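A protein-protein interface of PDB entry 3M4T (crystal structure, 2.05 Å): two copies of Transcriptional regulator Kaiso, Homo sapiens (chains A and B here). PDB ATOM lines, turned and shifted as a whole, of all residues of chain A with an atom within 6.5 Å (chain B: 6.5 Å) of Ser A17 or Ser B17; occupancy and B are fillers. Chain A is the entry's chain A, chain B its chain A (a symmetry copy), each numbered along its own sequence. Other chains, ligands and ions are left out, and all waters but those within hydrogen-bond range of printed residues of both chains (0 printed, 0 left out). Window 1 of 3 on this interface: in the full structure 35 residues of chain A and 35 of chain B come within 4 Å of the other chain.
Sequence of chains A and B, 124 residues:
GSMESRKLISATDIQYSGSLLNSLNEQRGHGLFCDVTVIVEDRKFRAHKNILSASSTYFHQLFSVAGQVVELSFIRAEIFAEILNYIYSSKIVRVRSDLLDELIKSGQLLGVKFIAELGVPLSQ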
ATOM      1  N   ASP A  13     -12.037 -14.854 -10.832  1.00  0.00           N
ATOM      2  CA  ASP A  13     -11.348 -16.082 -10.529  1.00  0.00           C
ATOM      3  C   ASP A  13      -9.851 -15.749 -10.406  1.00  0.00           C
ATOM      4  O   ASP A  13      -9.141 -15.696 -11.409  1.00  0.00           O
ATOM      5  CB  ASP A  13     -11.550 -17.072 -11.658  1.00  0.00           C
ATOM      6  CG  ASP A  13     -10.863 -18.371 -11.406  1.00  0.00           C
ATOM      7  OD1 ASP A  13     -10.216 -18.535 -10.349  1.00  0.00           O
ATOM      8  OD2 ASP A  13     -10.949 -19.247 -12.258  1.00  0.00           O
ATOM      9  N   ILE A  14      -9.377 -15.508  -9.188  1.00  0.00           N
ATOM     10  CA  ILE A  14      -7.941 -15.165  -9.015  1.00  0.00           C
ATOM     11  C   ILE A  14      -6.927 -16.309  -9.343  1.00  0.00           C
ATOM     12  O   ILE A  14      -5.721 -16.088  -9.507  1.00  0.00           O
ATOM     13  CB  ILE A  14      -7.694 -14.514  -7.644  1.00  0.00           C
ATOM     14  CG1 ILE A  14      -6.291 -13.905  -7.621  1.00  0.00           C
ATOM     15  CG2 ILE A  14      -7.891 -15.575  -6.519  1.00  0.00           C
ATOM     16  CD1 ILE A  14      -6.127 -12.594  -6.802  1.00  0.00           C
ATOM     17  N   GLN A  15      -7.411 -17.533  -9.453  1.00  0.00           N
ATOM     18  CA  GLN A  15      -6.533 -18.635  -9.820  1.00  0.00           C
ATOM     19  C   GLN A  15      -6.450 -18.859 -11.333  1.00  0.00           C
ATOM     20  O   GLN A  15      -5.623 -19.651 -11.790  1.00  0.00           O
ATOM     21  CB  GLN A  15      -6.993 -19.895  -9.101  1.00  0.00           C
ATOM     22  CG  GLN A  15      -7.073 -19.594  -7.596  1.00  0.00           C
ATOM     23  CD  GLN A  15      -7.535 -20.745  -6.785  1.00  0.00           C
ATOM     24  OE1 GLN A  15      -8.740 -20.906  -6.538  1.00  0.00           O
ATOM     25  NE2 GLN A  15      -6.592 -21.548  -6.321  1.00  0.00           N
ATOM     26  N   TYR A  16      -7.316 -18.191 -12.095  1.00  0.00           N
ATOM     27  CA  TYR A  16      -7.390 -18.441 -13.569  1.00  0.00           C
ATOM     28  C   TYR A  16      -6.050 -18.238 -14.315  1.00  0.00           C
ATOM     29  O   TYR A  16      -5.595 -19.103 -15.033  1.00  0.00           O
ATOM     30  CB  TYR A  16      -8.530 -17.625 -14.210  1.00  0.00           C
ATOM     31  CG  TYR A  16      -8.703 -17.929 -15.688  1.00  0.00           C
ATOM     32  CD1 TYR A  16      -9.142 -19.199 -16.146  1.00  0.00           C
ATOM     33  CD2 TYR A  16      -8.392 -16.967 -16.627  1.00  0.00           C
ATOM     34  CE1 TYR A  16      -9.246 -19.460 -17.554  1.00  0.00           C
ATOM     35  CE2 TYR A  16      -8.526 -17.205 -18.021  1.00  0.00           C
ATOM     36  CZ  TYR A  16      -8.943 -18.438 -18.459  1.00  0.00           C
ATOM     37  OH  TYR A  16      -9.010 -18.591 -19.820  1.00  0.00           O
ATOM     38  N   SER A  17      -5.420 -17.085 -14.121  1.00  0.00           N
ATOM     39  CA  SER A  17      -4.133 -16.758 -14.755  1.00  0.00           C
ATOM     40  C   SER A  17      -3.046 -17.801 -14.670  1.00  0.00           C
ATOM     41  O   SER A  17      -2.444 -18.159 -15.683  1.00  0.00           O
ATOM     42  CB  SER A  17      -3.595 -15.489 -14.098  1.00  0.00           C
ATOM     43  OG  SER A  17      -4.461 -14.443 -14.524  1.00  0.00           O
ATOM     44  N   GLY A  18      -2.781 -18.267 -13.449  1.00  0.00           N
ATOM     45  CA  GLY A  18      -1.647 -19.153 -13.177  1.00  0.00           C
ATOM     46  C   GLY A  18      -1.896 -20.462 -13.855  1.00  0.00           C
ATOM     47  O   GLY A  18      -0.992 -21.049 -14.448  1.00  0.00           O
ATOM     48  N   SER A  19      -3.151 -20.908 -13.761  1.00  0.00           N
ATOM     49  CA  SER A  19      -3.579 -22.116 -14.405  1.00  0.00           C
ATOM     50  C   SER A  19      -3.542 -21.984 -15.910  1.00  0.00           C
ATOM     51  O   SER A  19      -3.030 -22.869 -16.586  1.00  0.00           O
ATOM     52  CB  SER A  19      -4.983 -22.493 -13.926  1.00  0.00           C
ATOM     53  OG  SER A  19      -5.324 -23.726 -14.494  1.00  0.00           O
ATOM     54  N   LEU A  20      -4.050 -20.874 -16.448  1.00  0.00           N
ATOM     55  CA  LEU A  20      -3.989 -20.672 -17.890  1.00  0.00           C
ATOM     56  C   LEU A  20      -2.527 -20.697 -18.413  1.00  0.00           C
ATOM     57  O   LEU A  20      -2.239 -21.372 -19.341  1.00  0.00           O
ATOM     58  CB  LEU A  20      -4.643 -19.339 -18.276  1.00  0.00           C
ATOM     59  CG  LEU A  20      -4.605 -18.984 -19.770  1.00  0.00           C
ATOM     60  CD1 LEU A  20      -5.575 -19.858 -20.576  1.00  0.00           C
ATOM     61  CD2 LEU A  20      -4.992 -17.499 -19.970  1.00  0.00           C
ATOM     62  N   LEU A  21      -1.638 -19.942 -17.781  1.00  0.00           N
ATOM     63  CA  LEU A  21      -0.244 -19.851 -18.192  1.00  0.00           C
ATOM     64  C   LEU A  21       0.465 -21.182 -18.134  1.00  0.00           C
ATOM     65  O   LEU A  21       1.234 -21.508 -19.032  1.00  0.00           O
ATOM     66  CB  LEU A  21       0.473 -18.837 -17.292  1.00  0.00           C
ATOM     67  CG  LEU A  21       0.218 -17.392 -17.713  1.00  0.00           C
ATOM     68  CD1 LEU A  21       0.773 -16.422 -16.690  1.00  0.00           C
ATOM     69  CD2 LEU A  21       0.939 -17.170 -19.079  1.00  0.00           C
ATOM     70  N   ASN A  22       0.206 -21.965 -17.075  1.00  0.00           N
ATOM     71  CA  ASN A  22       0.814 -23.282 -16.962  1.00  0.00           C
ATOM     72  C   ASN A  22       0.389 -24.205 -18.091  1.00  0.00           C
ATOM     73  O   ASN A  22       1.226 -24.925 -18.671  1.00  0.00           O
ATOM     74  CB  ASN A  22       0.506 -23.939 -15.605  1.00  0.00           C
ATOM     75  CG  ASN A  22       1.102 -25.342 -15.526  1.00  0.00           C
ATOM     76  OD1 ASN A  22       2.338 -25.518 -15.613  1.00  0.00           O
ATOM     77  ND2 ASN A  22       0.239 -26.349 -15.450  1.00  0.00           N
ATOM     78  N   SER A  89       4.777 -17.618 -17.843  1.00  0.00           N
ATOM     79  CA  SER A  89       4.694 -17.904 -16.396  1.00  0.00           C
ATOM     80  C   SER A  89       4.495 -16.683 -15.508  1.00  0.00           C
ATOM     81  O   SER A  89       3.987 -16.844 -14.420  1.00  0.00           O
ATOM     82  CB  SER A  89       5.935 -18.659 -15.885  1.00  0.00           C
ATOM     83  OG  SER A  89       7.022 -17.735 -15.803  1.00  0.00           O
ATOM     84  N   SER A  90       4.918 -15.496 -15.962  1.00  0.00           N
ATOM     85  CA  SER A  90       4.983 -14.226 -15.167  1.00  0.00           C
ATOM     86  C   SER A  90       6.240 -14.097 -14.302  1.00  0.00           C
ATOM     87  O   SER A  90       6.423 -13.064 -13.660  1.00  0.00           O
ATOM     88  CB  SER A  90       3.691 -13.960 -14.309  1.00  0.00           C
ATOM     89  OG  SER A  90       3.780 -14.635 -13.049  1.00  0.00           O
ATOM     90  N   ASP B  13       6.052 -11.126 -11.683  1.00  0.00           N
ATOM     91  CA  ASP B  13       5.366  -9.948 -12.149  1.00  0.00           C
ATOM     92  C   ASP B  13       3.862 -10.168 -11.905  1.00  0.00           C
ATOM     93  O   ASP B  13       3.184 -10.785 -12.724  1.00  0.00           O
ATOM     94  CB  ASP B  13       5.612  -9.768 -13.633  1.00  0.00           C
ATOM     95  CG  ASP B  13       4.930  -8.562 -14.181  1.00  0.00           C
ATOM     96  OD1 ASP B  13       4.252  -7.834 -13.422  1.00  0.00           O
ATOM     97  OD2 ASP B  13       5.050  -8.320 -15.375  1.00  0.00           O
ATOM     98  N   ILE B  14       3.349  -9.682 -10.779  1.00  0.00           N
ATOM     99  CA  ILE B  14       1.905  -9.881 -10.487  1.00  0.00           C
ATOM    100  C   ILE B  14       0.913  -9.133 -11.435  1.00  0.00           C
ATOM    101  O   ILE B  14      -0.290  -9.419 -11.482  1.00  0.00           O
ATOM    102  CB  ILE B  14       1.610  -9.645  -8.996  1.00  0.00           C
ATOM    103  CG1 ILE B  14       0.202 -10.148  -8.677  1.00  0.00           C
ATOM    104  CG2 ILE B  14       1.782  -8.132  -8.663  1.00  0.00           C
ATOM    105  CD1 ILE B  14       0.000 -10.767  -7.265  1.00  0.00           C
ATOM    106  N   GLN B  15       1.411  -8.181 -12.203  1.00  0.00           N
ATOM    107  CA  GLN B  15       0.555  -7.488 -13.156  1.00  0.00           C
ATOM    108  C   GLN B  15       0.522  -8.159 -14.532  1.00  0.00           C
ATOM    109  O   GLN B  15      -0.283  -7.773 -15.382  1.00  0.00           O
ATOM    110  CB  GLN B  15       1.005  -6.038 -13.261  1.00  0.00           C
ATOM    111  CG  GLN B  15       1.036  -5.434 -11.848  1.00  0.00           C
ATOM    112  CD  GLN B  15       1.484  -4.022 -11.817  1.00  0.00           C
ATOM    113  OE1 GLN B  15       2.682  -3.737 -11.667  1.00  0.00           O
ATOM    114  NE2 GLN B  15       0.535  -3.106 -11.917  1.00  0.00           N
ATOM    115  N   TYR B  16       1.405  -9.133 -14.756  1.00  0.00           N
ATOM    116  CA  TYR B  16       1.526  -9.759 -16.110  1.00  0.00           C
ATOM    117  C   TYR B  16       0.208 -10.362 -16.651  1.00  0.00           C
ATOM    118  O   TYR B  16      -0.217 -10.058 -17.746  1.00  0.00           O
ATOM    119  CB  TYR B  16       2.677 -10.784 -16.141  1.00  0.00           C
ATOM    120  CG  TYR B  16       2.899 -11.367 -17.526  1.00  0.00           C
ATOM    121  CD1 TYR B  16       3.363 -10.575 -18.609  1.00  0.00           C
ATOM    122  CD2 TYR B  16       2.607 -12.695 -17.765  1.00  0.00           C
ATOM    123  CE1 TYR B  16       3.513 -11.155 -19.913  1.00  0.00           C
ATOM    124  CE2 TYR B  16       2.787 -13.285 -19.045  1.00  0.00           C
ATOM    125  CZ  TYR B  16       3.228 -12.512 -20.090  1.00  0.00           C
ATOM    126  OH  TYR B  16       3.339 -13.155 -21.296  1.00  0.00           O
ATOM    127  N   SER B  17      -0.439 -11.209 -15.859  1.00  0.00           N
ATOM    128  CA  SER B  17      -1.709 -11.849 -16.236  1.00  0.00           C
ATOM    129  C   SER B  17      -2.788 -10.951 -16.789  1.00  0.00           C
ATOM    130  O   SER B  17      -3.355 -11.235 -17.844  1.00  0.00           O
ATOM    131  CB  SER B  17      -2.279 -12.529 -14.994  1.00  0.00           C
ATOM    132  OG  SER B  17      -1.410 -13.625 -14.726  1.00  0.00           O
ATOM    133  N   GLY B  18      -3.086  -9.879 -16.054  1.00  0.00           N
ATOM    134  CA  GLY B  18      -4.219  -9.005 -16.366  1.00  0.00           C
ATOM    135  C   GLY B  18      -3.937  -8.306 -17.657  1.00  0.00           C
ATOM    136  O   GLY B  18      -4.817  -8.167 -18.506  1.00  0.00           O
ATOM    137  N   SER B  19      -2.682  -7.874 -17.793  1.00  0.00           N
ATOM    138  CA  SER B  19      -2.222  -7.238 -18.994  1.00  0.00           C
ATOM    139  C   SER B  19      -2.214  -8.198 -20.161  1.00  0.00           C
ATOM    140  O   SER B  19      -2.696  -7.855 -21.235  1.00  0.00           O
ATOM    141  CB  SER B  19      -0.830  -6.642 -18.769  1.00  0.00           C
ATOM    142  OG  SER B  19      -0.461  -5.943 -19.924  1.00  0.00           O
ATOM    143  N   LEU B  20      -1.701  -9.413 -19.961  1.00  0.00           N
ATOM    144  CA  LEU B  20      -1.719 -10.395 -21.037  1.00  0.00           C
ATOM    145  C   LEU B  20      -3.164 -10.684 -21.528  1.00  0.00           C
ATOM    146  O   LEU B  20      -3.417 -10.655 -22.683  1.00  0.00           O
ATOM    147  CB  LEU B  20      -1.066 -11.707 -20.582  1.00  0.00           C
ATOM    148  CG  LEU B  20      -1.061 -12.845 -21.613  1.00  0.00           C
ATOM    149  CD1 LEU B  20      -0.059 -12.570 -22.742  1.00  0.00           C
ATOM    150  CD2 LEU B  20      -0.683 -14.178 -20.926  1.00  0.00           C
ATOM    151  N   LEU B  21      -4.079 -10.958 -20.607  1.00  0.00           N
ATOM    152  CA  LEU B  21      -5.461 -11.279 -20.937  1.00  0.00           C
ATOM    153  C   LEU B  21      -6.158 -10.155 -21.664  1.00  0.00           C
ATOM    154  O   LEU B  21      -6.896 -10.401 -22.611  1.00  0.00           O
ATOM    155  CB  LEU B  21      -6.214 -11.613 -19.644  1.00  0.00           C
ATOM    156  CG  LEU B  21      -5.961 -13.040 -19.166  1.00  0.00           C
ATOM    157  CD1 LEU B  21      -6.556 -13.267 -17.792  1.00  0.00           C
ATOM    158  CD2 LEU B  21      -6.642 -14.002 -20.188  1.00  0.00           C
ATOM    159  N   ASN B  22      -5.925  -8.907 -21.226  1.00  0.00           N
ATOM    160  CA  ASN B  22      -6.523  -7.764 -21.896  1.00  0.00           C
ATOM    161  C   ASN B  22      -6.055  -7.637 -23.335  1.00  0.00           C
ATOM    162  O   ASN B  22      -6.867  -7.379 -24.246  1.00  0.00           O
ATOM    163  CB  ASN B  22      -6.251  -6.451 -21.139  1.00  0.00           C
ATOM    164  CG  ASN B  22      -6.835  -5.256 -21.886  1.00  0.00           C
ATOM    165  OD1 ASN B  22      -8.067  -5.171 -22.095  1.00  0.00           O
ATOM    166  ND2 ASN B  22      -5.966  -4.374 -22.366  1.00  0.00           N
ATOM    167  N   SER B  89     -10.512 -12.971 -19.541  1.00  0.00           N
ATOM    168  CA  SER B  89     -10.470 -11.917 -18.508  1.00  0.00           C
ATOM    169  C   SER B  89     -10.310 -12.419 -17.079  1.00  0.00           C
ATOM    170  O   SER B  89      -9.835 -11.666 -16.258  1.00  0.00           O
ATOM    171  CB  SER B  89     -11.719 -11.016 -18.552  1.00  0.00           C
ATOM    172  OG  SER B  89     -12.816 -11.742 -17.995  1.00  0.00           O
ATOM    173  N   SER B  90     -10.730 -13.659 -16.795  1.00  0.00           N
ATOM    174  CA  SER B  90     -10.831 -14.257 -15.424  1.00  0.00           C
ATOM    175  C   SER B  90     -12.115 -13.887 -14.677  1.00  0.00           C
ATOM    176  O   SER B  90     -12.329 -14.378 -13.569  1.00  0.00           O
ATOM    177  CB  SER B  90      -9.570 -13.980 -14.527  1.00  0.00           C
ATOM    178  OG  SER B  90      -9.690 -12.711 -13.873  1.00  0.00           O
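OG of Ser B17 sits close to OG of Ser A17 (3.2 Å).
N of Asp A13 is in hydrogen-bond range of O of Ser B90, at 2.8 Å.
The backbone carbonyl oxygen (O) of Ser A90 lies within hydrogen-bond range of the backbone NH (N) of Asp B13, 2.8 Å away.
The side-chain carboxylate (OD1) of Asp A13 is in hydrogen-bond range of the backbone NH (N) of Gln A15 (3.1 Å).
The backbone NH (N) of Tyr B16 is in hydrogen-bond range of the side-chain carboxylate (OD1) of Asp B13 (3.4 Å).
The backbone NH (N) of Gln B15 sits at hydrogen-bond distance from the side-chain carboxylate (OD1) of Asp B13 (3.1 Å).
OD1 of Asp A13 is in hydrogen-bond range of N of Tyr A16.
Ser B90 touches Tyr A16 (CB to CB, 3.8 Å).
Leu A20 touches Leu B21.
Leu A21 touches Leu B20 (CD2 to CD2, 3.9 Å).
Ser A90 touches Tyr B16 (CB to CB, 3.8 Å).
Of the printed residues of chain B, Asp A13 touches Ser B90.
Ser A17 touches just one residue of chain B: Ser B17 (2.9 Å).
Of the printed residues of chain B, Leu A20 touches Leu B21.
Of the printed residues of chain B, Leu A21 touches Leu B20.
Printed residues of chain A within 4 Å of Asp B13: Ser A90.
Ser B17 touches one residue of chain A.
Of the printed residues of chain A, Leu B20 touches Leu A21 (3.9 Å).
The nearest residue of chain B that does not touch Ser A17 is Leu B21 (4.1 Å).
Of the 12 printed residues of chain B, 6 touch a printed residue of chain A.
Of the 12 printed residues of chain A, 6 touch a printed residue of chain B.
Printed residues of chain A that touch a printed residue of chain B: Asp A13, Tyr A16, Ser A17, Leu A20, Leu A21 and Ser A90.
Among the printed residues, 7 pairs touch across the chains.
Asp A13 touches Ser B90, and with the chains exchanged Ser A90 touches Asp B13.
Tyr A16 touches Ser B90, and with the chains exchanged Ser A90 touches Tyr B16.
Ser A17 touches its own counterpart, Ser B17.
Leu A20 touches Leu B21, and with the chains exchanged Leu A21 touches Leu B20.
Positions printed for both chains: 13, 14, 15, 16, 17, 18, 19, 20, 21, 22, 89 and 90.
Of the 7 pairs that touch across the chains among the printed residues, 7 have their exchanged pair printed and touching as well.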
